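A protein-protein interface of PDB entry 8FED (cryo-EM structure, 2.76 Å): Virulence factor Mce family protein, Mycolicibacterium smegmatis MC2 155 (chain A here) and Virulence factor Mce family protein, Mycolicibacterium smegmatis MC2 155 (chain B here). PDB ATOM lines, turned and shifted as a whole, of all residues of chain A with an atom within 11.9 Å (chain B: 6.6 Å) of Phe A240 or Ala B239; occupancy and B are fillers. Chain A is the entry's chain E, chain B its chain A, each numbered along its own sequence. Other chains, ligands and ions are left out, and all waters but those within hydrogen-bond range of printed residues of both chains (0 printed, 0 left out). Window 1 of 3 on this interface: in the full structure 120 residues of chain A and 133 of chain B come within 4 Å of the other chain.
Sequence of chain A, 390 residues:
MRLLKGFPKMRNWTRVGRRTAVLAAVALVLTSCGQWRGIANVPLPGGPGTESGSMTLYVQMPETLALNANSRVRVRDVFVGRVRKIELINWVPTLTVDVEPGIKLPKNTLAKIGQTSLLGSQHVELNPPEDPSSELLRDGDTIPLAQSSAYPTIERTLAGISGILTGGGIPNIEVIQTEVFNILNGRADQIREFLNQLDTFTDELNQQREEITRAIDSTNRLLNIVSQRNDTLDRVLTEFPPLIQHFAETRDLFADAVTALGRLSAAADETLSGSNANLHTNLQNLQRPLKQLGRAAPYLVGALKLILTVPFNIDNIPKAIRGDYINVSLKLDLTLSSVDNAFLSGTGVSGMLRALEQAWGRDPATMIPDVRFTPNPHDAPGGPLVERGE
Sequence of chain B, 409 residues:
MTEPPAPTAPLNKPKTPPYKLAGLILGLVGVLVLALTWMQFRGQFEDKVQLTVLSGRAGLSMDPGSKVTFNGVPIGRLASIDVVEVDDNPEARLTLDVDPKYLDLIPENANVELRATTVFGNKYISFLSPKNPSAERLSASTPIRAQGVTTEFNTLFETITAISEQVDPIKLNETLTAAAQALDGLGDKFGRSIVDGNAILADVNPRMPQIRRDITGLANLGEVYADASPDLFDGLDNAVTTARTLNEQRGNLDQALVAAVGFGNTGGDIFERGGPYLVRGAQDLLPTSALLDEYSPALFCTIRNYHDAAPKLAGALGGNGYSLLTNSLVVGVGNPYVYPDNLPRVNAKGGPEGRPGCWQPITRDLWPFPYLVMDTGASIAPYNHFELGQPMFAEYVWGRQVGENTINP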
ATOM      1  N   ARG A 229      -1.262  36.670  27.226  1.00  0.00           N
ATOM      2  CA  ARG A 229      -2.306  36.028  26.432  1.00  0.00           C
ATOM      3  C   ARG A 229      -2.145  34.510  26.389  1.00  0.00           C
ATOM      4  O   ARG A 229      -2.710  33.852  25.506  1.00  0.00           O
ATOM      5  CB  ARG A 229      -2.347  36.597  25.012  1.00  0.00           C
ATOM      6  CG  ARG A 229      -2.373  38.111  24.943  1.00  0.00           C
ATOM      7  CD  ARG A 229      -3.634  38.671  25.574  1.00  0.00           C
ATOM      8  NE  ARG A 229      -3.708  40.120  25.449  1.00  0.00           N
ATOM      9  CZ  ARG A 229      -4.289  40.755  24.441  1.00  0.00           C
ATOM     10  NH1 ARG A 229      -4.877  40.096  23.456  1.00  0.00           N
ATOM     11  NH2 ARG A 229      -4.284  42.085  24.423  1.00  0.00           N
ATOM     12  N   ASP A 231      -3.504  32.415  28.147  1.00  0.00           N
ATOM     13  CA  ASP A 231      -4.830  31.806  28.201  1.00  0.00           C
ATOM     14  C   ASP A 231      -5.422  31.657  26.804  1.00  0.00           C
ATOM     15  O   ASP A 231      -5.997  30.612  26.468  1.00  0.00           O
ATOM     16  CB  ASP A 231      -5.755  32.636  29.090  1.00  0.00           C
ATOM     17  CG  ASP A 231      -5.321  32.639  30.542  1.00  0.00           C
ATOM     18  OD1 ASP A 231      -4.329  31.954  30.870  1.00  0.00           O
ATOM     19  OD2 ASP A 231      -5.971  33.327  31.356  1.00  0.00           O
ATOM     20  N   THR A 232      -5.280  32.694  25.975  1.00  0.00           N
ATOM     21  CA  THR A 232      -5.709  32.601  24.584  1.00  0.00           C
ATOM     22  C   THR A 232      -4.928  31.519  23.850  1.00  0.00           C
ATOM     23  O   THR A 232      -5.492  30.781  23.035  1.00  0.00           O
ATOM     24  CB  THR A 232      -5.531  33.954  23.894  1.00  0.00           C
ATOM     25  OG1 THR A 232      -6.384  34.924  24.514  1.00  0.00           O
ATOM     26  CG2 THR A 232      -5.870  33.861  22.413  1.00  0.00           C
ATOM     27  N   LEU A 233      -3.628  31.413  24.131  1.00  0.00           N
ATOM     28  CA  LEU A 233      -2.814  30.374  23.500  1.00  0.00           C
ATOM     29  C   LEU A 233      -3.318  28.979  23.851  1.00  0.00           C
ATOM     30  O   LEU A 233      -3.413  28.105  22.979  1.00  0.00           O
ATOM     31  CB  LEU A 233      -1.351  30.518  23.907  1.00  0.00           C
ATOM     32  CG  LEU A 233      -0.538  31.622  23.241  1.00  0.00           C
ATOM     33  CD1 LEU A 233       0.914  31.439  23.606  1.00  0.00           C
ATOM     34  CD2 LEU A 233      -0.722  31.590  21.736  1.00  0.00           C
ATOM     35  N   ASP A 234      -3.628  28.749  25.129  1.00  0.00           N
ATOM     36  CA  ASP A 234      -4.170  27.459  25.543  1.00  0.00           C
ATOM     37  C   ASP A 234      -5.507  27.191  24.872  1.00  0.00           C
ATOM     38  O   ASP A 234      -5.766  26.075  24.407  1.00  0.00           O
ATOM     39  CB  ASP A 234      -4.321  27.399  27.063  1.00  0.00           C
ATOM     40  CG  ASP A 234      -3.014  27.117  27.773  1.00  0.00           C
ATOM     41  OD1 ASP A 234      -2.291  28.078  28.104  1.00  0.00           O
ATOM     42  OD2 ASP A 234      -2.710  25.928  28.004  1.00  0.00           O
ATOM     43  N   ARG A 235      -6.372  28.206  24.814  1.00  0.00           N
ATOM     44  CA  ARG A 235      -7.683  28.013  24.204  1.00  0.00           C
ATOM     45  C   ARG A 235      -7.565  27.747  22.706  1.00  0.00           C
ATOM     46  O   ARG A 235      -8.403  27.041  22.135  1.00  0.00           O
ATOM     47  CB  ARG A 235      -8.572  29.222  24.492  1.00  0.00           C
ATOM     48  CG  ARG A 235     -10.045  28.873  24.632  1.00  0.00           C
ATOM     49  CD  ARG A 235     -10.767  29.758  25.642  1.00  0.00           C
ATOM     50  NE  ARG A 235     -10.735  31.174  25.299  1.00  0.00           N
ATOM     51  CZ  ARG A 235      -9.935  32.064  25.868  1.00  0.00           C
ATOM     52  NH1 ARG A 235      -9.075  31.716  26.813  1.00  0.00           N
ATOM     53  NH2 ARG A 235     -10.001  33.335  25.486  1.00  0.00           N
ATOM     54  N   VAL A 236      -6.534  28.300  22.061  1.00  0.00           N
ATOM     55  CA  VAL A 236      -6.283  28.009  20.652  1.00  0.00           C
ATOM     56  C   VAL A 236      -5.810  26.572  20.486  1.00  0.00           C
ATOM     57  O   VAL A 236      -6.337  25.814  19.663  1.00  0.00           O
ATOM     58  CB  VAL A 236      -5.260  29.001  20.070  1.00  0.00           C
ATOM     59  CG1 VAL A 236      -4.738  28.500  18.735  1.00  0.00           C
ATOM     60  CG2 VAL A 236      -5.875  30.376  19.903  1.00  0.00           C
ATOM     61  N   LEU A 237      -4.804  26.173  21.265  1.00  0.00           N
ATOM     62  CA  LEU A 237      -4.226  24.846  21.098  1.00  0.00           C
ATOM     63  C   LEU A 237      -5.150  23.732  21.572  1.00  0.00           C
ATOM     64  O   LEU A 237      -4.906  22.569  21.236  1.00  0.00           O
ATOM     65  CB  LEU A 237      -2.886  24.765  21.828  1.00  0.00           C
ATOM     66  CG  LEU A 237      -1.771  25.615  21.215  1.00  0.00           C
ATOM     67  CD1 LEU A 237      -0.511  25.555  22.059  1.00  0.00           C
ATOM     68  CD2 LEU A 237      -1.482  25.160  19.795  1.00  0.00           C
ATOM     69  N   THR A 238      -6.198  24.053  22.333  1.00  0.00           N
ATOM     70  CA  THR A 238      -7.149  23.024  22.739  1.00  0.00           C
ATOM     71  C   THR A 238      -8.202  22.733  21.675  1.00  0.00           C
ATOM     72  O   THR A 238      -8.739  21.621  21.641  1.00  0.00           O
ATOM     73  CB  THR A 238      -7.854  23.425  24.037  1.00  0.00           C
ATOM     74  OG1 THR A 238      -8.273  24.792  23.954  1.00  0.00           O
ATOM     75  CG2 THR A 238      -6.941  23.238  25.235  1.00  0.00           C
ATOM     76  N   GLU A 239      -8.514  23.694  20.804  1.00  0.00           N
ATOM     77  CA  GLU A 239      -9.676  23.562  19.929  1.00  0.00           C
ATOM     78  C   GLU A 239      -9.411  23.788  18.447  1.00  0.00           C
ATOM     79  O   GLU A 239     -10.246  23.376  17.633  1.00  0.00           O
ATOM     80  CB  GLU A 239     -10.789  24.522  20.376  1.00  0.00           C
ATOM     81  CG  GLU A 239     -11.305  24.245  21.780  1.00  0.00           C
ATOM     82  CD  GLU A 239     -12.309  25.275  22.252  1.00  0.00           C
ATOM     83  OE1 GLU A 239     -12.907  25.957  21.396  1.00  0.00           O
ATOM     84  OE2 GLU A 239     -12.494  25.408  23.479  1.00  0.00           O
ATOM     85  N   PHE A 240      -8.303  24.417  18.058  1.00  0.00           N
ATOM     86  CA  PHE A 240      -8.008  24.617  16.642  1.00  0.00           C
ATOM     87  C   PHE A 240      -7.432  23.383  15.939  1.00  0.00           C
ATOM     88  O   PHE A 240      -7.796  23.147  14.778  1.00  0.00           O
ATOM     89  CB  PHE A 240      -7.065  25.811  16.464  1.00  0.00           C
ATOM     90  CG  PHE A 240      -7.726  27.018  15.872  1.00  0.00           C
ATOM     91  CD1 PHE A 240      -8.765  26.877  14.968  1.00  0.00           C
ATOM     92  CD2 PHE A 240      -7.314  28.292  16.220  1.00  0.00           C
ATOM     93  CE1 PHE A 240      -9.376  27.985  14.418  1.00  0.00           C
ATOM     94  CE2 PHE A 240      -7.924  29.404  15.675  1.00  0.00           C
ATOM     95  CZ  PHE A 240      -8.955  29.249  14.774  1.00  0.00           C
ATOM     96  N   PRO A 241      -6.517  22.611  16.539  1.00  0.00           N
ATOM     97  CA  PRO A 241      -5.988  21.421  15.842  1.00  0.00           C
ATOM     98  C   PRO A 241      -7.074  20.447  15.403  1.00  0.00           C
ATOM     99  O   PRO A 241      -6.970  19.902  14.294  1.00  0.00           O
ATOM    100  CB  PRO A 241      -5.045  20.793  16.878  1.00  0.00           C
ATOM    101  CG  PRO A 241      -4.545  21.944  17.632  1.00  0.00           C
ATOM    102  CD  PRO A 241      -5.701  22.902  17.738  1.00  0.00           C
ATOM    103  N   PRO A 242      -8.117  20.170  16.212  1.00  0.00           N
ATOM    104  CA  PRO A 242      -9.185  19.298  15.683  1.00  0.00           C
ATOM    105  C   PRO A 242      -9.892  19.880  14.470  1.00  0.00           C
ATOM    106  O   PRO A 242     -10.209  19.143  13.527  1.00  0.00           O
ATOM    107  CB  PRO A 242     -10.137  19.139  16.875  1.00  0.00           C
ATOM    108  CG  PRO A 242      -9.300  19.366  18.052  1.00  0.00           C
ATOM    109  CD  PRO A 242      -8.347  20.438  17.647  1.00  0.00           C
ATOM    110  N   LEU A 243     -10.144  21.191  14.471  1.00  0.00           N
ATOM    111  CA  LEU A 243     -10.793  21.828  13.330  1.00  0.00           C
ATOM    112  C   LEU A 243      -9.928  21.721  12.083  1.00  0.00           C
ATOM    113  O   LEU A 243     -10.422  21.400  10.995  1.00  0.00           O
ATOM    114  CB  LEU A 243     -11.093  23.292  13.649  1.00  0.00           C
ATOM    115  CG  LEU A 243     -11.667  24.115  12.496  1.00  0.00           C
ATOM    116  CD1 LEU A 243     -13.113  23.728  12.241  1.00  0.00           C
ATOM    117  CD2 LEU A 243     -11.540  25.602  12.772  1.00  0.00           C
ATOM    118  N   ILE A 244      -8.628  21.993  12.224  1.00  0.00           N
ATOM    119  CA  ILE A 244      -7.719  21.920  11.084  1.00  0.00           C
ATOM    120  C   ILE A 244      -7.627  20.489  10.570  1.00  0.00           C
ATOM    121  O   ILE A 244      -7.613  20.248   9.355  1.00  0.00           O
ATOM    122  CB  ILE A 244      -6.340  22.484  11.468  1.00  0.00           C
ATOM    123  CG1 ILE A 244      -6.455  23.975  11.787  1.00  0.00           C
ATOM    124  CG2 ILE A 244      -5.338  22.263  10.354  1.00  0.00           C
ATOM    125  CD1 ILE A 244      -5.138  24.637  12.115  1.00  0.00           C
ATOM    126  N   GLN A 245      -7.571  19.516  11.485  1.00  0.00           N
ATOM    127  CA  GLN A 245      -7.516  18.115  11.083  1.00  0.00           C
ATOM    128  C   GLN A 245      -8.767  17.709  10.316  1.00  0.00           C
ATOM    129  O   GLN A 245      -8.678  17.035   9.281  1.00  0.00           O
ATOM    130  CB  GLN A 245      -7.325  17.228  12.313  1.00  0.00           C
ATOM    131  CG  GLN A 245      -7.486  15.746  12.043  1.00  0.00           C
ATOM    132  CD  GLN A 245      -7.250  14.903  13.280  1.00  0.00           C
ATOM    133  OE1 GLN A 245      -6.477  15.280  14.162  1.00  0.00           O
ATOM    134  NE2 GLN A 245      -7.920  13.760  13.354  1.00  0.00           N
ATOM    135  N   HIS A 246      -9.944  18.118  10.796  1.00  0.00           N
ATOM    136  CA  HIS A 246     -11.169  17.757  10.091  1.00  0.00           C
ATOM    137  C   HIS A 246     -11.261  18.458   8.742  1.00  0.00           C
ATOM    138  O   HIS A 246     -11.746  17.870   7.770  1.00  0.00           O
ATOM    139  CB  HIS A 246     -12.400  18.076  10.933  1.00  0.00           C
ATOM    140  CG  HIS A 246     -13.668  17.520  10.363  1.00  0.00           C
ATOM    141  ND1 HIS A 246     -13.946  16.171  10.347  1.00  0.00           N
ATOM    142  CD2 HIS A 246     -14.722  18.128   9.770  1.00  0.00           C
ATOM    143  CE1 HIS A 246     -15.121  15.972   9.779  1.00  0.00           C
ATOM    144  NE2 HIS A 246     -15.613  17.144   9.419  1.00  0.00           N
ATOM    145  N   PHE A 247     -10.809  19.714   8.661  1.00  0.00           N
ATOM    146  CA  PHE A 247     -10.776  20.402   7.372  1.00  0.00           C
ATOM    147  C   PHE A 247      -9.871  19.672   6.390  1.00  0.00           C
ATOM    148  O   PHE A 247     -10.217  19.518   5.213  1.00  0.00           O
ATOM    149  CB  PHE A 247     -10.316  21.849   7.549  1.00  0.00           C
ATOM    150  CG  PHE A 247     -11.405  22.786   7.985  1.00  0.00           C
ATOM    151  CD1 PHE A 247     -12.728  22.379   7.998  1.00  0.00           C
ATOM    152  CD2 PHE A 247     -11.105  24.083   8.368  1.00  0.00           C
ATOM    153  CE1 PHE A 247     -13.730  23.243   8.394  1.00  0.00           C
ATOM    154  CE2 PHE A 247     -12.103  24.951   8.765  1.00  0.00           C
ATOM    155  CZ  PHE A 247     -13.416  24.531   8.776  1.00  0.00           C
ATOM    156  N   ALA A 248      -8.705  19.222   6.857  1.00  0.00           N
ATOM    157  CA  ALA A 248      -7.821  18.425   6.014  1.00  0.00           C
ATOM    158  C   ALA A 248      -8.469  17.108   5.610  1.00  0.00           C
ATOM    159  O   ALA A 248      -8.183  16.583   4.528  1.00  0.00           O
ATOM    160  CB  ALA A 248      -6.501  18.164   6.735  1.00  0.00           C
ATOM    161  N   GLU A 249      -9.331  16.555   6.465  1.00  0.00           N
ATOM    162  CA  GLU A 249     -10.048  15.335   6.105  1.00  0.00           C
ATOM    163  C   GLU A 249     -11.029  15.572   4.962  1.00  0.00           C
ATOM    164  O   GLU A 249     -11.219  14.694   4.112  1.00  0.00           O
ATOM    165  CB  GLU A 249     -10.781  14.774   7.325  1.00  0.00           C
ATOM    166  CG  GLU A 249      -9.876  14.158   8.379  1.00  0.00           C
ATOM    167  CD  GLU A 249      -9.391  12.772   8.002  1.00  0.00           C
ATOM    168  OE1 GLU A 249      -9.970  12.167   7.075  1.00  0.00           O
ATOM    169  OE2 GLU A 249      -8.430  12.286   8.635  1.00  0.00           O
ATOM    170  N   ASP B 234      -6.740  38.786  20.077  1.00  0.00           N
ATOM    171  CA  ASP B 234      -8.189  38.972  20.133  1.00  0.00           C
ATOM    172  C   ASP B 234      -8.879  38.191  19.020  1.00  0.00           C
ATOM    173  O   ASP B 234      -9.901  37.518  19.249  1.00  0.00           O
ATOM    174  CB  ASP B 234      -8.533  40.458  20.045  1.00  0.00           C
ATOM    175  CG  ASP B 234      -7.892  41.272  21.151  1.00  0.00           C
ATOM    176  OD1 ASP B 234      -7.117  40.695  21.943  1.00  0.00           O
ATOM    177  OD2 ASP B 234      -8.161  42.487  21.231  1.00  0.00           O
ATOM    178  N   GLY B 235      -8.329  38.266  17.803  1.00  0.00           N
ATOM    179  CA  GLY B 235      -8.854  37.473  16.712  1.00  0.00           C
ATOM    180  C   GLY B 235      -8.765  35.986  16.973  1.00  0.00           C
ATOM    181  O   GLY B 235      -9.648  35.234  16.575  1.00  0.00           O
ATOM    182  N   LEU B 236      -7.707  35.544  17.656  1.00  0.00           N
ATOM    183  CA  LEU B 236      -7.579  34.130  17.992  1.00  0.00           C
ATOM    184  C   LEU B 236      -8.622  33.702  19.016  1.00  0.00           C
ATOM    185  O   LEU B 236      -9.151  32.592  18.933  1.00  0.00           O
ATOM    186  CB  LEU B 236      -6.170  33.830  18.502  1.00  0.00           C
ATOM    187  CG  LEU B 236      -5.077  33.703  17.439  1.00  0.00           C
ATOM    188  CD1 LEU B 236      -3.746  33.350  18.082  1.00  0.00           C
ATOM    189  CD2 LEU B 236      -5.463  32.670  16.393  1.00  0.00           C
ATOM    190  N   ASP B 237      -8.930  34.563  19.989  1.00  0.00           N
ATOM    191  CA  ASP B 237      -9.997  34.257  20.942  1.00  0.00           C
ATOM    192  C   ASP B 237     -11.335  34.082  20.233  1.00  0.00           C
ATOM    193  O   ASP B 237     -12.035  33.072  20.414  1.00  0.00           O
ATOM    194  CB  ASP B 237     -10.097  35.367  21.988  1.00  0.00           C
ATOM    195  CG  ASP B 237      -9.047  35.249  23.065  1.00  0.00           C
ATOM    196  OD1 ASP B 237      -8.882  34.141  23.614  1.00  0.00           O
ATOM    197  OD2 ASP B 237      -8.382  36.263  23.363  1.00  0.00           O
ATOM    198  N   ASN B 238     -11.704  35.062  19.409  1.00  0.00           N
ATOM    199  CA  ASN B 238     -12.978  34.963  18.703  1.00  0.00           C
ATOM    200  C   ASN B 238     -12.968  33.823  17.685  1.00  0.00           C
ATOM    201  O   ASN B 238     -14.010  33.199  17.430  1.00  0.00           O
ATOM    202  CB  ASN B 238     -13.305  36.300  18.049  1.00  0.00           C
ATOM    203  CG  ASN B 238     -13.483  37.412  19.064  1.00  0.00           C
ATOM    204  OD1 ASN B 238     -14.084  37.211  20.119  1.00  0.00           O
ATOM    205  ND2 ASN B 238     -12.954  38.589  18.755  1.00  0.00           N
ATOM    206  N   ALA B 239     -11.801  33.521  17.116  1.00  0.00           N
ATOM    207  CA  ALA B 239     -11.676  32.393  16.208  1.00  0.00           C
ATOM    208  C   ALA B 239     -11.822  31.073  16.944  1.00  0.00           C
ATOM    209  O   ALA B 239     -12.331  30.110  16.374  1.00  0.00           O
ATOM    210  CB  ALA B 239     -10.337  32.455  15.476  1.00  0.00           C
ATOM    211  N   VAL B 240     -11.387  31.006  18.203  1.00  0.00           N
ATOM    212  CA  VAL B 240     -11.646  29.820  19.012  1.00  0.00           C
ATOM    213  C   VAL B 240     -13.136  29.675  19.268  1.00  0.00           C
ATOM    214  O   VAL B 240     -13.680  28.564  19.240  1.00  0.00           O
ATOM    215  CB  VAL B 240     -10.850  29.880  20.327  1.00  0.00           C
ATOM    216  CG1 VAL B 240     -11.341  28.823  21.293  1.00  0.00           C
ATOM    217  CG2 VAL B 240      -9.395  29.662  20.049  1.00  0.00           C
ATOM    218  N   THR B 241     -13.818  30.794  19.528  1.00  0.00           N
ATOM    219  CA  THR B 241     -15.271  30.745  19.689  1.00  0.00           C
ATOM    220  C   THR B 241     -15.943  30.151  18.450  1.00  0.00           C
ATOM    221  O   THR B 241     -16.697  29.169  18.539  1.00  0.00           O
ATOM    222  CB  THR B 241     -15.817  32.144  19.978  1.00  0.00           C
ATOM    223  OG1 THR B 241     -15.217  32.658  21.173  1.00  0.00           O
ATOM    224  CG2 THR B 241     -17.326  32.099  20.155  1.00  0.00           C
ATOM    225  N   THR B 242     -15.643  30.708  17.273  1.00  0.00           N
ATOM    226  CA  THR B 242     -16.275  30.197  16.058  1.00  0.00           C
ATOM    227  C   THR B 242     -15.755  28.814  15.671  1.00  0.00           C
ATOM    228  O   THR B 242     -16.470  28.061  15.003  1.00  0.00           O
ATOM    229  CB  THR B 242     -16.102  31.177  14.893  1.00  0.00           C
ATOM    230  OG1 THR B 242     -16.832  30.697  13.756  1.00  0.00           O
ATOM    231  CG2 THR B 242     -14.651  31.318  14.510  1.00  0.00           C
ATOM    232  N   ALA B 243     -14.551  28.440  16.111  1.00  0.00           N
ATOM    233  CA  ALA B 243     -14.025  27.115  15.815  1.00  0.00           C
ATOM    234  C   ALA B 243     -14.714  26.053  16.656  1.00  0.00           C
ATOM    235  O   ALA B 243     -14.987  24.952  16.170  1.00  0.00           O
ATOM    236  CB  ALA B 243     -12.515  27.089  16.045  1.00  0.00           C
ATOM    237  N   ARG B 244     -14.991  26.360  17.925  1.00  0.00           N
ATOM    238  CA  ARG B 244     -15.830  25.478  18.726  1.00  0.00           C
ATOM    239  C   ARG B 244     -17.225  25.381  18.128  1.00  0.00           C
ATOM    240  O   ARG B 244     -17.829  24.299  18.114  1.00  0.00           O
ATOM    241  CB  ARG B 244     -15.896  25.977  20.170  1.00  0.00           C
ATOM    242  CG  ARG B 244     -16.822  25.166  21.064  1.00  0.00           C
ATOM    243  CD  ARG B 244     -16.935  25.775  22.452  1.00  0.00           C
ATOM    244  NE  ARG B 244     -15.706  25.629  23.224  1.00  0.00           N
ATOM    245  CZ  ARG B 244     -15.471  24.639  24.073  1.00  0.00           C
ATOM    246  NH1 ARG B 244     -16.361  23.682  24.284  1.00  0.00           N
ATOM    247  NH2 ARG B 244     -14.317  24.609  24.732  1.00  0.00           N
ATOM    248  N   ASN B 247     -16.840  23.008  15.204  1.00  0.00           N
ATOM    249  CA  ASN B 247     -16.588  21.646  15.664  1.00  0.00           C
ATOM    250  C   ASN B 247     -17.854  20.996  16.207  1.00  0.00           C
ATOM    251  O   ASN B 247     -18.074  19.796  16.007  1.00  0.00           O
ATOM    252  CB  ASN B 247     -15.490  21.640  16.727  1.00  0.00           C
ATOM    253  CG  ASN B 247     -14.123  21.940  16.152  1.00  0.00           C
ATOM    254  OD1 ASN B 247     -13.810  21.543  15.031  1.00  0.00           O
ATOM    255  ND2 ASN B 247     -13.299  22.642  16.919  1.00  0.00           N
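The backbone carbonyl oxygen (O) of Asp B234 is in hydrogen-bond range of the side-chain amide nitrogen (ND2) of Asn B238 (3.3 Å). O of Asp B237 lies within hydrogen-bond range of OG1 of Thr B241 (3.3 Å). The backbone carbonyl oxygen (O) of Ala B243 sits at hydrogen-bond distance from the side-chain amide nitrogen (ND2) of Asn B247 (3.0 Å). The backbone carbonyl oxygen (O) of Asp A231 sits at hydrogen-bond distance from the guanidinium group (NH1) of Arg A235, 3.3 Å away. The backbone carbonyl oxygen (O) of Arg A235 lies within hydrogen-bond range of the side-chain hydroxyl (OG1) of Thr A238, 2.9 Å away.
The side-chain carboxylate (OD1) of Asp B234 lies within salt-bridge range of the guanidinium group (NH1) of Arg A229. The side-chain carboxylate of Asp B237 sits at hydrogen-bond distance from the side-chain hydroxyl of Thr A232. NE of Arg A235 is in salt-bridge range of OD1 of Asp B237. The guanidinium group of Arg B244 lies within salt-bridge range of the side-chain carboxylate of Glu A239 (3.2 Å). The side-chain amide nitrogen (ND2) of Asn B247 lies within hydrogen-bond range of the backbone carbonyl oxygen (O) of Glu A239 (3.2 Å). OE1 of Glu A239 sits close to O of Val B240, at 3.5 Å.
Among the printed residues, pairs that only touch across the chains: Leu A243 with Asn B247 (3.5 Å), Arg A235 with Val B240 (3.5 Å), Phe A240 with Ala B239 (3.6 Å), Val A236 with Val B240 (3.6 Å), Phe A240 with Ala B243 (3.6 Å), Leu A243 with Ala B243 (3.7 Å), Val A236 with Leu B236 (3.7 Å) and Thr A232 with Leu B236 (3.9 Å).
Asp A234 touches none of the printed residues of chain B. Printed residues of chain B within 4 Å of Arg A235: Asp B237 (2.3 Å) and Val B240 (3.5 Å). Ala A248 touches none of the printed residues of chain B. Gly B235 touches none of the printed residues of chain A. Of chain A, only Thr A232 and Val A236 come within 4 Å of Leu B236. Asp B237 touches just these residues of chain A: Thr A232 and Arg A235. No residue of chain A comes within 4 Å of Asn B238. Ala B239 touches just one residue of chain A: Phe A240 (3.6 Å). No residue of chain A comes within 4 Å of Thr B241. Ala B243 touches just these residues of chain A: Phe A240 (3.6 Å) and Leu A243 (3.7 Å). Printed residues of chain A within 4 Å of Arg B244: Glu A239. Printed residues of chain A within 4 Å of Asn B247: Glu A239 and Leu A243. The nearest residue of chain B that does not touch Phe A240 is Leu B236 (4.2 Å). The nearest printed residue of chain B that does not touch Arg A229 is Asp B237 (5.2 Å).
Printed residues of chain A that touch a printed residue of chain B: Arg A229, Thr A232, Arg A235, Val A236, Glu A239, Phe A240 and Leu A243. Hydrophobic or aromatic side chains of chain A within 4 Å of the printed part of chain B: Val A236, Phe A240 and Leu A243. Of the 12 printed residues of chain B, 8 touch a printed residue of chain A. Hydrophobic or aromatic side chains of chain B within 4 Å of the printed part of chain A: Leu B236, Ala B239, Val B240 and Ala B243. Along chain B the printed residues that touch a printed residue of chain A span positions 234 to 247. Among the printed residues, 14 pairs touch across the chains. Among the printed residues, Asp or Glu carboxylates within 4 Å of a Lys or Arg side-chain nitrogen of the other chain: Arg A229 with Asp B234 (2.8 Å), Arg A235 with Asp B237 (2.3 Å) and Glu A239 with Arg B244 (2.4 Å).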
